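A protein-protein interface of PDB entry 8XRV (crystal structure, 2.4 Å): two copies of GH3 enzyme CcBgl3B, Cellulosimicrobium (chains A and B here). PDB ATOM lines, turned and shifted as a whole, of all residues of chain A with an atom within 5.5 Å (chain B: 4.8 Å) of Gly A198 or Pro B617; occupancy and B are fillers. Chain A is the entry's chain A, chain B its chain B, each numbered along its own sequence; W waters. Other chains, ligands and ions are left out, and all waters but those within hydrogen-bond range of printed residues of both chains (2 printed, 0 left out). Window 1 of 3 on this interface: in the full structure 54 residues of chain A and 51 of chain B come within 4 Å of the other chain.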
ATOM      1  N   ASP A 144      20.737  18.554 -23.246  1.00  0.00           N
ATOM      2  CA  ASP A 144      19.625  18.340 -24.170  1.00  0.00           C
ATOM      3  C   ASP A 144      19.451  19.624 -24.967  1.00  0.00           C
ATOM      4  O   ASP A 144      19.185  20.694 -24.398  1.00  0.00           O
ATOM      5  CB  ASP A 144      18.337  17.952 -23.427  1.00  0.00           C
ATOM      6  CG  ASP A 144      17.226  17.397 -24.365  1.00  0.00           C
ATOM      7  OD1 ASP A 144      17.050  17.890 -25.509  1.00  0.00           O
ATOM      8  OD2 ASP A 144      16.521  16.444 -23.936  1.00  0.00           O
ATOM      9  N   ARG A 146      17.198  20.541 -26.937  1.00  0.00           N
ATOM     10  CA  ARG A 146      15.845  21.077 -26.969  1.00  0.00           C
ATOM     11  C   ARG A 146      15.636  22.161 -25.922  1.00  0.00           C
ATOM     12  O   ARG A 146      14.774  23.039 -26.100  1.00  0.00           O
ATOM     13  CB  ARG A 146      14.837  19.941 -26.757  1.00  0.00           C
ATOM     14  CG  ARG A 146      14.843  18.902 -27.871  1.00  0.00           C
ATOM     15  CD  ARG A 146      13.856  17.809 -27.576  1.00  0.00           C
ATOM     16  NE  ARG A 146      14.341  16.987 -26.487  1.00  0.00           N
ATOM     17  CZ  ARG A 146      13.662  15.998 -25.919  1.00  0.00           C
ATOM     18  NH1 ARG A 146      14.216  15.318 -24.920  1.00  0.00           N
ATOM     19  NH2 ARG A 146      12.436  15.693 -26.343  1.00  0.00           N
ATOM     20  N   THR A 196      16.061  17.939 -17.959  1.00  0.00           N
ATOM     21  CA  THR A 196      14.753  17.522 -17.484  1.00  0.00           C
ATOM     22  C   THR A 196      14.019  16.848 -18.636  1.00  0.00           C
ATOM     23  O   THR A 196      14.436  16.935 -19.791  1.00  0.00           O
ATOM     24  CB  THR A 196      13.948  18.726 -16.959  1.00  0.00           C
ATOM     25  OG1 THR A 196      13.859  19.730 -17.985  1.00  0.00           O
ATOM     26  CG2 THR A 196      14.628  19.356 -15.724  1.00  0.00           C
ATOM     27  N   GLN A 197      12.901  16.202 -18.314  1.00  0.00           N
ATOM     28  CA  GLN A 197      12.129  15.435 -19.295  1.00  0.00           C
ATOM     29  C   GLN A 197      11.743  16.277 -20.507  1.00  0.00           C
ATOM     30  O   GLN A 197      11.173  17.369 -20.370  1.00  0.00           O
ATOM     31  CB  GLN A 197      10.854  14.879 -18.645  1.00  0.00           C
ATOM     32  CG  GLN A 197      11.100  13.915 -17.497  1.00  0.00           C
ATOM     33  CD  GLN A 197       9.832  13.236 -17.010  1.00  0.00           C
ATOM     34  OE1 GLN A 197       8.711  13.634 -17.364  1.00  0.00           O
ATOM     35  NE2 GLN A 197      10.002  12.203 -16.188  1.00  0.00           N
ATOM     36  N   GLY A 198      12.011  15.738 -21.696  1.00  0.00           N
ATOM     37  CA  GLY A 198      11.635  16.398 -22.926  1.00  0.00           C
ATOM     38  C   GLY A 198      12.468  17.595 -23.289  1.00  0.00           C
ATOM     39  O   GLY A 198      12.152  18.283 -24.269  1.00  0.00           O
ATOM     40  N   GLY A 199      13.520  17.871 -22.533  1.00  0.00           N
ATOM     41  CA  GLY A 199      14.181  19.150 -22.670  1.00  0.00           C
ATOM     42  C   GLY A 199      13.300  20.324 -22.317  1.00  0.00           C
ATOM     43  O   GLY A 199      13.592  21.456 -22.723  1.00  0.00           O
ATOM     44  N   ARG A 200      12.203  20.082 -21.605  1.00  0.00           N
ATOM     45  CA  ARG A 200      11.269  21.150 -21.285  1.00  0.00           C
ATOM     46  C   ARG A 200      11.776  21.964 -20.096  1.00  0.00           C
ATOM     47  O   ARG A 200      12.723  21.585 -19.408  1.00  0.00           O
ATOM     48  CB  ARG A 200       9.895  20.558 -21.016  1.00  0.00           C
ATOM     49  CG  ARG A 200       9.422  19.730 -22.195  1.00  0.00           C
ATOM     50  CD  ARG A 200       8.380  18.721 -21.780  1.00  0.00           C
ATOM     51  NE  ARG A 200       7.943  17.950 -22.929  1.00  0.00           N
ATOM     52  CZ  ARG A 200       7.036  16.977 -22.894  1.00  0.00           C
ATOM     53  NH1 ARG A 200       6.434  16.641 -21.751  1.00  0.00           N
ATOM     54  NH2 ARG A 200       6.723  16.345 -24.014  1.00  0.00           N
ATOM     55  N   SER A 203      10.438  20.641 -16.146  1.00  0.00           N
ATOM     56  CA  SER A 203       9.765  19.368 -15.944  1.00  0.00           C
ATOM     57  C   SER A 203      10.608  18.556 -14.954  1.00  0.00           C
ATOM     58  O   SER A 203      11.634  19.020 -14.448  1.00  0.00           O
ATOM     59  CB  SER A 203       9.578  18.662 -17.284  1.00  0.00           C
ATOM     60  OG  SER A 203      10.810  18.653 -17.999  1.00  0.00           O
ATOM     61  N   SER A 531      11.362  25.993 -24.918  1.00  0.00           N
ATOM     62  CA  SER A 531      12.086  24.871 -25.464  1.00  0.00           C
ATOM     63  C   SER A 531      11.606  24.601 -26.888  1.00  0.00           C
ATOM     64  O   SER A 531      10.490  24.959 -27.278  1.00  0.00           O
ATOM     65  CB  SER A 531      11.901  23.634 -24.567  1.00  0.00           C
ATOM     66  OG  SER A 531      12.503  23.844 -23.290  1.00  0.00           O
ATOM     67  N   GLY B 614      11.407  14.707 -31.252  1.00  0.00           N
ATOM     68  CA  GLY B 614      11.768  15.686 -30.247  1.00  0.00           C
ATOM     69  C   GLY B 614      10.644  16.057 -29.323  1.00  0.00           C
ATOM     70  O   GLY B 614      10.892  16.718 -28.308  1.00  0.00           O
ATOM     71  N   GLN B 615       9.418  15.636 -29.646  1.00  0.00           N
ATOM     72  CA  GLN B 615       8.257  15.950 -28.827  1.00  0.00           C
ATOM     73  C   GLN B 615       8.229  15.132 -27.550  1.00  0.00           C
ATOM     74  O   GLN B 615       7.573  15.532 -26.586  1.00  0.00           O
ATOM     75  CB  GLN B 615       6.982  15.709 -29.635  1.00  0.00           C
ATOM     76  CG  GLN B 615       5.772  16.381 -29.081  1.00  0.00           C
ATOM     77  CD  GLN B 615       4.495  15.862 -29.696  1.00  0.00           C
ATOM     78  OE1 GLN B 615       4.389  14.672 -30.010  1.00  0.00           O
ATOM     79  NE2 GLN B 615       3.506  16.747 -29.862  1.00  0.00           N
ATOM     80  N   GLN B 616       8.958  14.025 -27.516  1.00  0.00           N
ATOM     81  CA  GLN B 616       8.894  13.094 -26.399  1.00  0.00           C
ATOM     82  C   GLN B 616       9.383  13.730 -25.094  1.00  0.00           C
ATOM     83  O   GLN B 616      10.282  14.576 -25.107  1.00  0.00           O
ATOM     84  CB  GLN B 616       9.742  11.886 -26.718  1.00  0.00           C
ATOM     85  CG  GLN B 616       9.130  11.020 -27.775  1.00  0.00           C
ATOM     86  CD  GLN B 616       9.741   9.648 -27.738  1.00  0.00           C
ATOM     87  OE1 GLN B 616       9.133   8.696 -27.228  1.00  0.00           O
ATOM     88  NE2 GLN B 616      10.981   9.541 -28.239  1.00  0.00           N
ATOM     89  N   PRO B 617       8.864  13.279 -23.935  1.00  0.00           N
ATOM     90  CA  PRO B 617       7.931  12.157 -23.748  1.00  0.00           C
ATOM     91  C   PRO B 617       6.468  12.472 -24.063  1.00  0.00           C
ATOM     92  O   PRO B 617       5.942  13.561 -23.755  1.00  0.00           O
ATOM     93  CB  PRO B 617       8.085  11.828 -22.265  1.00  0.00           C
ATOM     94  CG  PRO B 617       8.407  13.132 -21.631  1.00  0.00           C
ATOM     95  CD  PRO B 617       9.196  13.930 -22.649  1.00  0.00           C
ATOM     96  N   THR B 618       5.816  11.488 -24.684  1.00  0.00           N
ATOM     97  CA  THR B 618       4.441  11.617 -25.114  1.00  0.00           C
ATOM     98  C   THR B 618       3.509  10.609 -24.465  1.00  0.00           C
ATOM     99  O   THR B 618       2.312  10.636 -24.752  1.00  0.00           O
ATOM    100  CB  THR B 618       4.340  11.526 -26.651  1.00  0.00           C
ATOM    101  OG1 THR B 618       5.137  10.435 -27.152  1.00  0.00           O
ATOM    102  CG2 THR B 618       4.762  12.838 -27.292  1.00  0.00           C
ATOM    103  N   TYR B 619       3.999   9.756 -23.575  1.00  0.00           N
ATOM    104  CA  TYR B 619       3.083   8.956 -22.790  1.00  0.00           C
ATOM    105  C   TYR B 619       2.137   9.860 -21.980  1.00  0.00           C
ATOM    106  O   TYR B 619       2.413  11.038 -21.711  1.00  0.00           O
ATOM    107  CB  TYR B 619       3.848   7.989 -21.879  1.00  0.00           C
ATOM    108  CG  TYR B 619       4.999   8.578 -21.103  1.00  0.00           C
ATOM    109  CD1 TYR B 619       4.771   9.352 -19.958  1.00  0.00           C
ATOM    110  CD2 TYR B 619       6.313   8.339 -21.483  1.00  0.00           C
ATOM    111  CE1 TYR B 619       5.815   9.877 -19.237  1.00  0.00           C
ATOM    112  CE2 TYR B 619       7.379   8.860 -20.759  1.00  0.00           C
ATOM    113  CZ  TYR B 619       7.117   9.642 -19.630  1.00  0.00           C
ATOM    114  OH  TYR B 619       8.150  10.185 -18.881  1.00  0.00           O
ATOM    115  N   VAL B 622       2.508  11.918 -17.776  1.00  0.00           N
ATOM    116  CA  VAL B 622       3.632  12.820 -17.523  1.00  0.00           C
ATOM    117  C   VAL B 622       3.502  13.491 -16.159  1.00  0.00           C
ATOM    118  O   VAL B 622       2.419  13.911 -15.737  1.00  0.00           O
ATOM    119  CB  VAL B 622       3.759  13.857 -18.656  1.00  0.00           C
ATOM    120  CG1 VAL B 622       4.679  14.989 -18.252  1.00  0.00           C
ATOM    121  CG2 VAL B 622       4.420  13.189 -19.857  1.00  0.00           C
ATOM    122  N   TYR B 631       6.206  23.335 -26.770  1.00  0.00           N
ATOM    123  CA  TYR B 631       7.467  23.753 -27.367  1.00  0.00           C
ATOM    124  C   TYR B 631       7.213  24.997 -28.206  1.00  0.00           C
ATOM    125  O   TYR B 631       6.146  25.164 -28.797  1.00  0.00           O
ATOM    126  CB  TYR B 631       8.085  22.650 -28.246  1.00  0.00           C
ATOM    127  CG  TYR B 631       8.546  21.431 -27.485  1.00  0.00           C
ATOM    128  CD1 TYR B 631       9.795  21.402 -26.852  1.00  0.00           C
ATOM    129  CD2 TYR B 631       7.731  20.307 -27.387  1.00  0.00           C
ATOM    130  CE1 TYR B 631      10.217  20.273 -26.144  1.00  0.00           C
ATOM    131  CE2 TYR B 631       8.132  19.179 -26.674  1.00  0.00           C
ATOM    132  CZ  TYR B 631       9.368  19.161 -26.061  1.00  0.00           C
ATOM    133  OH  TYR B 631       9.760  18.031 -25.370  1.00  0.00           O
HETATM  134  O   HOH W   1       7.791  10.257 -15.777  1.00  0.00           O
HETATM  135  O   HOH W   2       6.650  12.359 -16.783  1.00  0.00           O
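The guanidinium group (NH2) of Arg A146 is in hydrogen-bond range of the backbone carbonyl oxygen (O) of Gly B614 (2.7 Å).
The guanidinium group (NH2) of Arg A146 sits at hydrogen-bond distance from the backbone carbonyl oxygen (O) of Gln B616 (2.7 Å).
The backbone carbonyl oxygen (O) of Gly A198 is in hydrogen-bond range of the side-chain hydroxyl (OH) of Tyr B631, 2.6 Å away.
The guanidinium group (NH2) of Arg A200 lies within hydrogen-bond range of the backbone carbonyl oxygen (O) of Gln B615.
The backbone carbonyl oxygen (O) of Pro B617 sits at hydrogen-bond distance from the guanidinium group (NH2) of Arg A200.
The guanidinium group (NE) of Arg A200 sits at hydrogen-bond distance from the side-chain hydroxyl (OH) of Tyr B631 (3.0 Å).
NH1 of Arg A146 is in salt-bridge range of OD2 of Asp A144, 2.7 Å away.
NH2 of Arg A146 sits close to O of Gly A198.
The side-chain hydroxyl of Thr A196 is in hydrogen-bond range of the backbone carbonyl oxygen of Arg A200 (2.6 Å).
The backbone carbonyl oxygen of Gln A197 lies within hydrogen-bond range of the side-chain hydroxyl of Ser A203 (2.7 Å).
The backbone carbonyl oxygen of Gly A199 lies within hydrogen-bond range of the side-chain hydroxyl of Ser A531, 2.7 Å away.
The backbone carbonyl oxygen of Gly B614 sits at hydrogen-bond distance from the side-chain hydroxyl of Tyr B631.
Among the printed residues, pairs that only touch across the chains: Arg A146 with Tyr B631, Gln A197 with Tyr B619, Gly A198 with Gln B616, Gly A198 with Pro B617, Arg A200 with Gln B616 and Ser A531 with Tyr B631.
Of the printed residues of chain B, Gly A198 touches Gln B616 (3.1 Å), Pro B617 (3.5 Å) and Tyr B631 (2.6 Å).
Pro B617 touches just these residues of chain A: Gly A198 (3.5 Å) and Arg A200 (2.9 Å).
Of the printed residues of chain A, Gln B615 touches Arg A200.
Of the printed residues of chain A, Gln B616 touches Arg A146 (2.7 Å), Gly A198 (3.1 Å) and Arg A200 (3.9 Å).
The nearest residue of chain B that does not touch Gly A198 is Gly B614 (4.5 Å).
Hydrophobic or aromatic side chains of chain B within 4 Å of the printed part of chain A: Pro B617, Tyr B619 and Tyr B631.
Along chain B the printed residues that touch a printed residue of chain A span positions 614 to 631.
Among the printed residues, 12 pairs touch across the chains.
Among the printed residues, no Asp or Glu carboxylate lies within 4 Å of a Lys or Arg side-chain nitrogen of the other chain.
No position is printed for both chains.
Of the 12 pairs that touch across the chains among the printed residues, none has its exchanged pair printed and touching as well.
Water W2 lies within hydrogen-bond range of the side-chain amide oxygen (OE1) of Gln A197 (2.5 Å) and the side-chain hydroxyl (OH) of Tyr B619 (3.4 Å).
Water W1 lies within hydrogen-bond range of the side-chain amide nitrogen of Gln A197 (3.0 Å) and the side-chain hydroxyl of Tyr B619 (3.1 Å).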
